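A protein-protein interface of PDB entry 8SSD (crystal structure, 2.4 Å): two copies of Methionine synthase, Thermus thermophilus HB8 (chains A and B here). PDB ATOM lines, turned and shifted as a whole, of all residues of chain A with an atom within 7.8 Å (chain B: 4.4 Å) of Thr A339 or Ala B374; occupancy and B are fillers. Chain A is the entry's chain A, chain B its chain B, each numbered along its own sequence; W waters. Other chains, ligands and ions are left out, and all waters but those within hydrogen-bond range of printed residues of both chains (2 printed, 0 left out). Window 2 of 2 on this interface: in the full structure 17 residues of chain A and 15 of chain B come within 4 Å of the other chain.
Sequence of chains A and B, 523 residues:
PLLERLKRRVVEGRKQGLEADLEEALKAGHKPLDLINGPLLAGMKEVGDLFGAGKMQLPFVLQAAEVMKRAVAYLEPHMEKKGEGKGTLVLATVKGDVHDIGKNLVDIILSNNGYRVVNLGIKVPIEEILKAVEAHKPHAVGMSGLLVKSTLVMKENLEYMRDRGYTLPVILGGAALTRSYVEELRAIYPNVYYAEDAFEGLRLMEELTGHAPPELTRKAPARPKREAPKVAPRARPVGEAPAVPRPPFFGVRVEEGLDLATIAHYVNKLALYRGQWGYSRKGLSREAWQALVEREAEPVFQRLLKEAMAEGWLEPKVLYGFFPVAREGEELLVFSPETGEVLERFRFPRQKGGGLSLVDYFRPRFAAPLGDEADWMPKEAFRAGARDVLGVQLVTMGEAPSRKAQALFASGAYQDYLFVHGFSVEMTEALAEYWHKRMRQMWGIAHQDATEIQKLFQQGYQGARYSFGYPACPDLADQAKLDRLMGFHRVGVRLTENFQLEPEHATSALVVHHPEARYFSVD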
ATOM      1  N   PHE A 335     -16.158  -3.434 -16.107  1.00  0.00           N
ATOM      2  CA  PHE A 335     -17.276  -3.229 -17.026  1.00  0.00           C
ATOM      3  C   PHE A 335     -17.264  -4.321 -18.087  1.00  0.00           C
ATOM      4  O   PHE A 335     -16.191  -4.796 -18.474  1.00  0.00           O
ATOM      5  CB  PHE A 335     -17.208  -1.864 -17.721  1.00  0.00           C
ATOM      6  CG  PHE A 335     -17.279  -0.670 -16.808  1.00  0.00           C
ATOM      7  CD1 PHE A 335     -16.173  -0.289 -16.053  1.00  0.00           C
ATOM      8  CD2 PHE A 335     -18.439   0.102 -16.724  1.00  0.00           C
ATOM      9  CE1 PHE A 335     -16.226   0.817 -15.217  1.00  0.00           C
ATOM     10  CE2 PHE A 335     -18.494   1.205 -15.877  1.00  0.00           C
ATOM     11  CZ  PHE A 335     -17.380   1.576 -15.147  1.00  0.00           C
ATOM     12  N   SER A 336     -18.468  -4.688 -18.568  1.00  0.00           N
ATOM     13  CA  SER A 336     -18.630  -5.608 -19.690  1.00  0.00           C
ATOM     14  C   SER A 336     -18.133  -4.944 -20.976  1.00  0.00           C
ATOM     15  O   SER A 336     -18.670  -3.887 -21.320  1.00  0.00           O
ATOM     16  CB  SER A 336     -20.060  -5.993 -19.871  1.00  0.00           C
ATOM     17  OG  SER A 336     -20.252  -6.783 -21.040  1.00  0.00           O
ATOM     18  N   PRO A 337     -17.204  -5.554 -21.767  1.00  0.00           N
ATOM     19  CA  PRO A 337     -16.850  -5.005 -23.078  1.00  0.00           C
ATOM     20  C   PRO A 337     -17.931  -5.079 -24.168  1.00  0.00           C
ATOM     21  O   PRO A 337     -17.732  -4.456 -25.213  1.00  0.00           O
ATOM     22  CB  PRO A 337     -15.613  -5.796 -23.517  1.00  0.00           C
ATOM     23  CG  PRO A 337     -15.330  -6.831 -22.448  1.00  0.00           C
ATOM     24  CD  PRO A 337     -16.520  -6.833 -21.519  1.00  0.00           C
ATOM     25  N   GLU A 338     -19.041  -5.822 -23.935  1.00  0.00           N
ATOM     26  CA  GLU A 338     -20.179  -5.911 -24.839  1.00  0.00           C
ATOM     27  C   GLU A 338     -21.280  -4.930 -24.452  1.00  0.00           C
ATOM     28  O   GLU A 338     -21.661  -4.114 -25.295  1.00  0.00           O
ATOM     29  CB  GLU A 338     -20.691  -7.353 -24.893  1.00  0.00           C
ATOM     30  CG  GLU A 338     -19.679  -8.315 -25.507  1.00  0.00           C
ATOM     31  CD  GLU A 338     -19.199  -8.000 -26.917  1.00  0.00           C
ATOM     32  OE1 GLU A 338     -20.018  -7.480 -27.736  1.00  0.00           O
ATOM     33  OE2 GLU A 338     -18.016  -8.268 -27.198  1.00  0.00           O
ATOM     34  N   THR A 339     -21.756  -5.006 -23.194  1.00  0.00           N
ATOM     35  CA  THR A 339     -22.896  -4.242 -22.701  1.00  0.00           C
ATOM     36  C   THR A 339     -22.509  -2.932 -22.015  1.00  0.00           C
ATOM     37  O   THR A 339     -23.367  -2.057 -21.939  1.00  0.00           O
ATOM     38  CB  THR A 339     -23.787  -5.081 -21.768  1.00  0.00           C
ATOM     39  OG1 THR A 339     -23.052  -5.460 -20.614  1.00  0.00           O
ATOM     40  CG2 THR A 339     -24.293  -6.366 -22.376  1.00  0.00           C
ATOM     41  N   GLY A 340     -21.289  -2.820 -21.455  1.00  0.00           N
ATOM     42  CA  GLY A 340     -20.915  -1.696 -20.593  1.00  0.00           C
ATOM     43  C   GLY A 340     -21.532  -1.730 -19.184  1.00  0.00           C
ATOM     44  O   GLY A 340     -21.444  -0.728 -18.472  1.00  0.00           O
ATOM     45  N   GLU A 341     -22.138  -2.862 -18.767  1.00  0.00           N
ATOM     46  CA  GLU A 341     -22.706  -3.037 -17.435  1.00  0.00           C
ATOM     47  C   GLU A 341     -21.560  -3.355 -16.481  1.00  0.00           C
ATOM     48  O   GLU A 341     -20.626  -4.075 -16.864  1.00  0.00           O
ATOM     49  CB  GLU A 341     -23.743  -4.167 -17.479  1.00  0.00           C
ATOM     50  CG  GLU A 341     -24.528  -4.439 -16.211  1.00  0.00           C
ATOM     51  CD  GLU A 341     -25.708  -5.351 -16.504  1.00  0.00           C
ATOM     52  OE1 GLU A 341     -26.726  -4.819 -16.983  1.00  0.00           O
ATOM     53  OE2 GLU A 341     -25.567  -6.590 -16.362  1.00  0.00           O
ATOM     54  N   VAL A 342     -21.655  -2.837 -15.239  1.00  0.00           N
ATOM     55  CA  VAL A 342     -20.699  -3.136 -14.177  1.00  0.00           C
ATOM     56  C   VAL A 342     -20.913  -4.594 -13.754  1.00  0.00           C
ATOM     57  O   VAL A 342     -21.958  -4.911 -13.187  1.00  0.00           O
ATOM     58  CB  VAL A 342     -20.824  -2.149 -12.995  1.00  0.00           C
ATOM     59  CG1 VAL A 342     -19.960  -2.541 -11.795  1.00  0.00           C
ATOM     60  CG2 VAL A 342     -20.479  -0.728 -13.452  1.00  0.00           C
ATOM     61  N   LEU A 343     -19.933  -5.464 -14.060  1.00  0.00           N
ATOM     62  CA  LEU A 343     -20.001  -6.888 -13.762  1.00  0.00           C
ATOM     63  C   LEU A 343     -19.560  -7.164 -12.329  1.00  0.00           C
ATOM     64  O   LEU A 343     -20.245  -7.912 -11.640  1.00  0.00           O
ATOM     65  CB  LEU A 343     -19.113  -7.653 -14.749  1.00  0.00           C
ATOM     66  CG  LEU A 343     -19.442  -7.480 -16.229  1.00  0.00           C
ATOM     67  CD1 LEU A 343     -18.583  -8.412 -17.070  1.00  0.00           C
ATOM     68  CD2 LEU A 343     -20.931  -7.714 -16.521  1.00  0.00           C
ATOM     69  N   PRO A 378     -14.216   0.111 -25.587  1.00  0.00           N
ATOM     70  CA  PRO A 378     -15.553  -0.353 -25.990  1.00  0.00           C
ATOM     71  C   PRO A 378     -16.653   0.672 -25.696  1.00  0.00           C
ATOM     72  O   PRO A 378     -16.613   1.303 -24.638  1.00  0.00           O
ATOM     73  CB  PRO A 378     -15.778  -1.645 -25.194  1.00  0.00           C
ATOM     74  CG  PRO A 378     -14.390  -2.116 -24.888  1.00  0.00           C
ATOM     75  CD  PRO A 378     -13.594  -0.851 -24.659  1.00  0.00           C
ATOM     76  N   LYS A 379     -17.592   0.812 -26.645  1.00  0.00           N
ATOM     77  CA  LYS A 379     -18.457   1.978 -26.785  1.00  0.00           C
ATOM     78  C   LYS A 379     -19.339   2.181 -25.552  1.00  0.00           C
ATOM     79  O   LYS A 379     -19.363   3.284 -25.005  1.00  0.00           O
ATOM     80  CB  LYS A 379     -19.343   1.834 -28.031  1.00  0.00           C
ATOM     81  CG  LYS A 379     -20.203   3.041 -28.408  1.00  0.00           C
ATOM     82  CD  LYS A 379     -21.054   2.800 -29.645  1.00  0.00           C
ATOM     83  CE  LYS A 379     -22.019   3.929 -29.945  1.00  0.00           C
ATOM     84  NZ  LYS A 379     -23.142   3.986 -28.974  1.00  0.00           N
ATOM     85  N   GLU A 380     -20.030   1.114 -25.124  1.00  0.00           N
ATOM     86  CA  GLU A 380     -20.973   1.178 -24.012  1.00  0.00           C
ATOM     87  C   GLU A 380     -20.253   1.324 -22.668  1.00  0.00           C
ATOM     88  O   GLU A 380     -20.752   2.053 -21.812  1.00  0.00           O
ATOM     89  CB  GLU A 380     -21.902  -0.038 -23.985  1.00  0.00           C
ATOM     90  CG  GLU A 380     -22.777  -0.165 -25.230  1.00  0.00           C
ATOM     91  CD  GLU A 380     -22.258  -0.974 -26.411  1.00  0.00           C
ATOM     92  OE1 GLU A 380     -21.061  -1.368 -26.414  1.00  0.00           O
ATOM     93  OE2 GLU A 380     -23.051  -1.194 -27.345  1.00  0.00           O
ATOM     94  N   ALA A 381     -19.124   0.611 -22.482  1.00  0.00           N
ATOM     95  CA  ALA A 381     -18.314   0.714 -21.269  1.00  0.00           C
ATOM     96  C   ALA A 381     -17.713   2.114 -21.101  1.00  0.00           C
ATOM     97  O   ALA A 381     -17.718   2.631 -19.984  1.00  0.00           O
ATOM     98  CB  ALA A 381     -17.234  -0.345 -21.263  1.00  0.00           C
ATOM     99  N   PHE A 382     -17.235   2.727 -22.205  1.00  0.00           N
ATOM    100  CA  PHE A 382     -16.765   4.111 -22.214  1.00  0.00           C
ATOM    101  C   PHE A 382     -17.892   5.101 -21.893  1.00  0.00           C
ATOM    102  O   PHE A 382     -17.639   6.052 -21.146  1.00  0.00           O
ATOM    103  CB  PHE A 382     -16.071   4.455 -23.538  1.00  0.00           C
ATOM    104  CG  PHE A 382     -15.362   5.788 -23.542  1.00  0.00           C
ATOM    105  CD1 PHE A 382     -16.046   6.960 -23.867  1.00  0.00           C
ATOM    106  CD2 PHE A 382     -14.017   5.884 -23.183  1.00  0.00           C
ATOM    107  CE1 PHE A 382     -15.402   8.194 -23.826  1.00  0.00           C
ATOM    108  CE2 PHE A 382     -13.369   7.112 -23.167  1.00  0.00           C
ATOM    109  CZ  PHE A 382     -14.063   8.267 -23.481  1.00  0.00           C
ATOM    110  N   ALA A 384     -20.626   4.330 -20.119  1.00  0.00           N
ATOM    111  CA  ALA A 384     -20.859   4.051 -18.700  1.00  0.00           C
ATOM    112  C   ALA A 384     -19.733   4.528 -17.766  1.00  0.00           C
ATOM    113  O   ALA A 384     -19.905   4.427 -16.550  1.00  0.00           O
ATOM    114  CB  ALA A 384     -21.105   2.570 -18.513  1.00  0.00           C
ATOM    115  N   ASP B 372     -24.446 -16.413 -17.173  1.00  0.00           N
ATOM    116  CA  ASP B 372     -23.845 -15.093 -17.344  1.00  0.00           C
ATOM    117  C   ASP B 372     -23.609 -14.748 -18.824  1.00  0.00           C
ATOM    118  O   ASP B 372     -22.683 -13.990 -19.119  1.00  0.00           O
ATOM    119  CB  ASP B 372     -22.574 -15.020 -16.481  1.00  0.00           C
ATOM    120  CG  ASP B 372     -21.377 -15.863 -16.910  1.00  0.00           C
ATOM    121  OD1 ASP B 372     -21.547 -16.805 -17.726  1.00  0.00           O
ATOM    122  OD2 ASP B 372     -20.263 -15.563 -16.419  1.00  0.00           O
ATOM    123  N   GLU B 373     -24.453 -15.241 -19.749  1.00  0.00           N
ATOM    124  CA  GLU B 373     -24.146 -15.197 -21.186  1.00  0.00           C
ATOM    125  C   GLU B 373     -24.342 -13.790 -21.758  1.00  0.00           C
ATOM    126  O   GLU B 373     -23.595 -13.428 -22.666  1.00  0.00           O
ATOM    127  CB  GLU B 373     -24.835 -16.275 -22.037  1.00  0.00           C
ATOM    128  CG  GLU B 373     -26.294 -16.546 -21.737  1.00  0.00           C
ATOM    129  CD  GLU B 373     -26.497 -17.709 -20.770  1.00  0.00           C
ATOM    130  OE1 GLU B 373     -25.888 -17.672 -19.673  1.00  0.00           O
ATOM    131  OE2 GLU B 373     -27.254 -18.657 -21.101  1.00  0.00           O
ATOM    132  N   ALA B 374     -25.256 -12.988 -21.178  1.00  0.00           N
ATOM    133  CA  ALA B 374     -25.411 -11.555 -21.429  1.00  0.00           C
ATOM    134  C   ALA B 374     -24.132 -10.721 -21.269  1.00  0.00           C
ATOM    135  O   ALA B 374     -23.984  -9.698 -21.941  1.00  0.00           O
ATOM    136  CB  ALA B 374     -26.495 -11.003 -20.523  1.00  0.00           C
ATOM    137  N   ASP B 375     -23.239 -11.131 -20.353  1.00  0.00           N
ATOM    138  CA  ASP B 375     -21.969 -10.461 -20.093  1.00  0.00           C
ATOM    139  C   ASP B 375     -20.957 -10.633 -21.234  1.00  0.00           C
ATOM    140  O   ASP B 375     -20.181  -9.700 -21.450  1.00  0.00           O
ATOM    141  CB  ASP B 375     -21.347 -10.947 -18.781  1.00  0.00           C
ATOM    142  CG  ASP B 375     -22.209 -10.763 -17.536  1.00  0.00           C
ATOM    143  OD1 ASP B 375     -23.106  -9.883 -17.545  1.00  0.00           O
ATOM    144  OD2 ASP B 375     -21.998 -11.515 -16.555  1.00  0.00           O
ATOM    145  N   TRP B 376     -20.938 -11.790 -21.930  1.00  0.00           N
ATOM    146  CA  TRP B 376     -19.899 -12.145 -22.909  1.00  0.00           C
ATOM    147  C   TRP B 376     -20.410 -12.433 -24.326  1.00  0.00           C
ATOM    148  O   TRP B 376     -19.590 -12.355 -25.239  1.00  0.00           O
ATOM    149  CB  TRP B 376     -19.035 -13.304 -22.386  1.00  0.00           C
ATOM    150  CG  TRP B 376     -19.774 -14.554 -22.003  1.00  0.00           C
ATOM    151  CD1 TRP B 376     -20.058 -14.947 -20.737  1.00  0.00           C
ATOM    152  CD2 TRP B 376     -20.253 -15.606 -22.863  1.00  0.00           C
ATOM    153  NE1 TRP B 376     -20.709 -16.147 -20.739  1.00  0.00           N
ATOM    154  CE2 TRP B 376     -20.845 -16.583 -22.025  1.00  0.00           C
ATOM    155  CE3 TRP B 376     -20.236 -15.844 -24.252  1.00  0.00           C
ATOM    156  CZ2 TRP B 376     -21.403 -17.769 -22.528  1.00  0.00           C
ATOM    157  CZ3 TRP B 376     -20.822 -17.001 -24.750  1.00  0.00           C
ATOM    158  CH2 TRP B 376     -21.386 -17.962 -23.894  1.00  0.00           C
ATOM    159  N   LYS B 379     -22.832  -8.236 -28.486  1.00  0.00           N
ATOM    160  CA  LYS B 379     -23.829  -7.328 -27.928  1.00  0.00           C
ATOM    161  C   LYS B 379     -25.091  -7.297 -28.786  1.00  0.00           C
ATOM    162  O   LYS B 379     -26.190  -7.475 -28.260  1.00  0.00           O
ATOM    163  CB  LYS B 379     -23.242  -5.914 -27.787  1.00  0.00           C
ATOM    164  CG  LYS B 379     -24.137  -4.814 -27.210  1.00  0.00           C
ATOM    165  CD  LYS B 379     -24.737  -5.157 -25.867  1.00  0.00           C
ATOM    166  CE  LYS B 379     -25.626  -4.108 -25.233  1.00  0.00           C
ATOM    167  NZ  LYS B 379     -25.104  -2.729 -25.325  1.00  0.00           N
ATOM    168  N   PHE B 382     -26.870 -10.841 -29.168  1.00  0.00           N
ATOM    169  CA  PHE B 382     -27.641 -11.076 -27.950  1.00  0.00           C
ATOM    170  C   PHE B 382     -28.914 -10.223 -27.901  1.00  0.00           C
ATOM    171  O   PHE B 382     -29.953 -10.745 -27.488  1.00  0.00           O
ATOM    172  CB  PHE B 382     -26.779 -10.876 -26.696  1.00  0.00           C
ATOM    173  CG  PHE B 382     -27.441 -11.322 -25.411  1.00  0.00           C
ATOM    174  CD1 PHE B 382     -28.267 -10.456 -24.695  1.00  0.00           C
ATOM    175  CD2 PHE B 382     -27.265 -12.621 -24.928  1.00  0.00           C
ATOM    176  CE1 PHE B 382     -28.894 -10.866 -23.520  1.00  0.00           C
ATOM    177  CE2 PHE B 382     -27.888 -13.031 -23.747  1.00  0.00           C
ATOM    178  CZ  PHE B 382     -28.708 -12.157 -23.048  1.00  0.00           C
HETATM  179  O   HOH W   1     -24.072  -7.489 -18.398  1.00  0.00           O
HETATM  180  O   HOH W   2     -24.785  -9.234 -15.312  1.00  0.00           O
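CG2 of Thr A339 touches O of Ala B374 (3.4 Å). Thr A339 touches Lys B379. CD2 of Leu A343 touches OD1 of Asp B375, at 3.2 Å.
Water W1 lies within hydrogen-bond range of OE2 of Glu A341 (2.7 Å), OD1 of Asp B375 (2.7 Å) and OG1 of Thr A339 (3.2 Å). Water W2 bridges the side-chain carboxylate of Asp B375 (2.9 Å) and the side-chain carboxylate of Glu A341 (3.0 Å).
2 positions are printed for both chains. Of the 6 pairs that touch across the chains among the printed residues, none has its exchanged pair printed and touching as well.
The side-chain hydroxyl (OG) of Ser A336 lies within hydrogen-bond range of the backbone carbonyl oxygen (O) of Asp B375, 2.9 Å away. OE1 of Glu A338 sits at hydrogen-bond distance from N of Lys B379, at 3.0 Å. OE2 of Glu A380 is in salt-bridge range of NZ of Lys B379 (3.3 Å).
OG of Ser A336 lies close to N of Glu A338 (3.3 Å). The backbone carbonyl oxygen of Glu A341 is in hydrogen-bond range of the backbone NH of Ser A336 (2.8 Å). OG1 of Thr A339 sits at hydrogen-bond distance from OG of Ser A336, at 3.1 Å. The backbone NH (N) of Glu A341 sits close to the side-chain hydroxyl (OG1) of Thr A339 (3.3 Å).
Of the 7 printed residues of chain B, 3 touch a printed residue of chain A. Printed residues of chain A that touch a printed residue of chain B: Ser A336, Glu A338, Thr A339, Leu A343 and Glu A380. Along chain A the printed residues that touch a printed residue of chain B span positions 336 to 380. Among the printed residues, 6 pairs touch across the chains. Among the printed residues, Asp or Glu carboxylates within 4 Å of a Lys or Arg side-chain nitrogen of the other chain: Glu A380 with Lys B379 (3.3 Å).
Of the printed residues of chain B, Ser A336 touches Asp B375. Thr A339 touches two residues of chain B. Of the printed residues of chain B, Leu A343 touches Asp B375 (3.2 Å). Of the printed residues of chain B, Glu A380 touches Lys B379 (3.3 Å). Glu B373 touches none of the printed residues of chain A. Of chain A, only Thr A339 comes within 4 Å of Ala B374. Of the printed residues of chain A, Asp B375 touches Ser A336 and Leu A343. Trp B376 touches none of the printed residues of chain A. Printed residues of chain A within 4 Å of Lys B379: Glu A338 (3.0 Å), Thr A339 (3.7 Å) and Glu A380 (3.3 Å). The nearest printed residue of chain B that does not touch Thr A339 is Asp B375 (5.1 Å).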
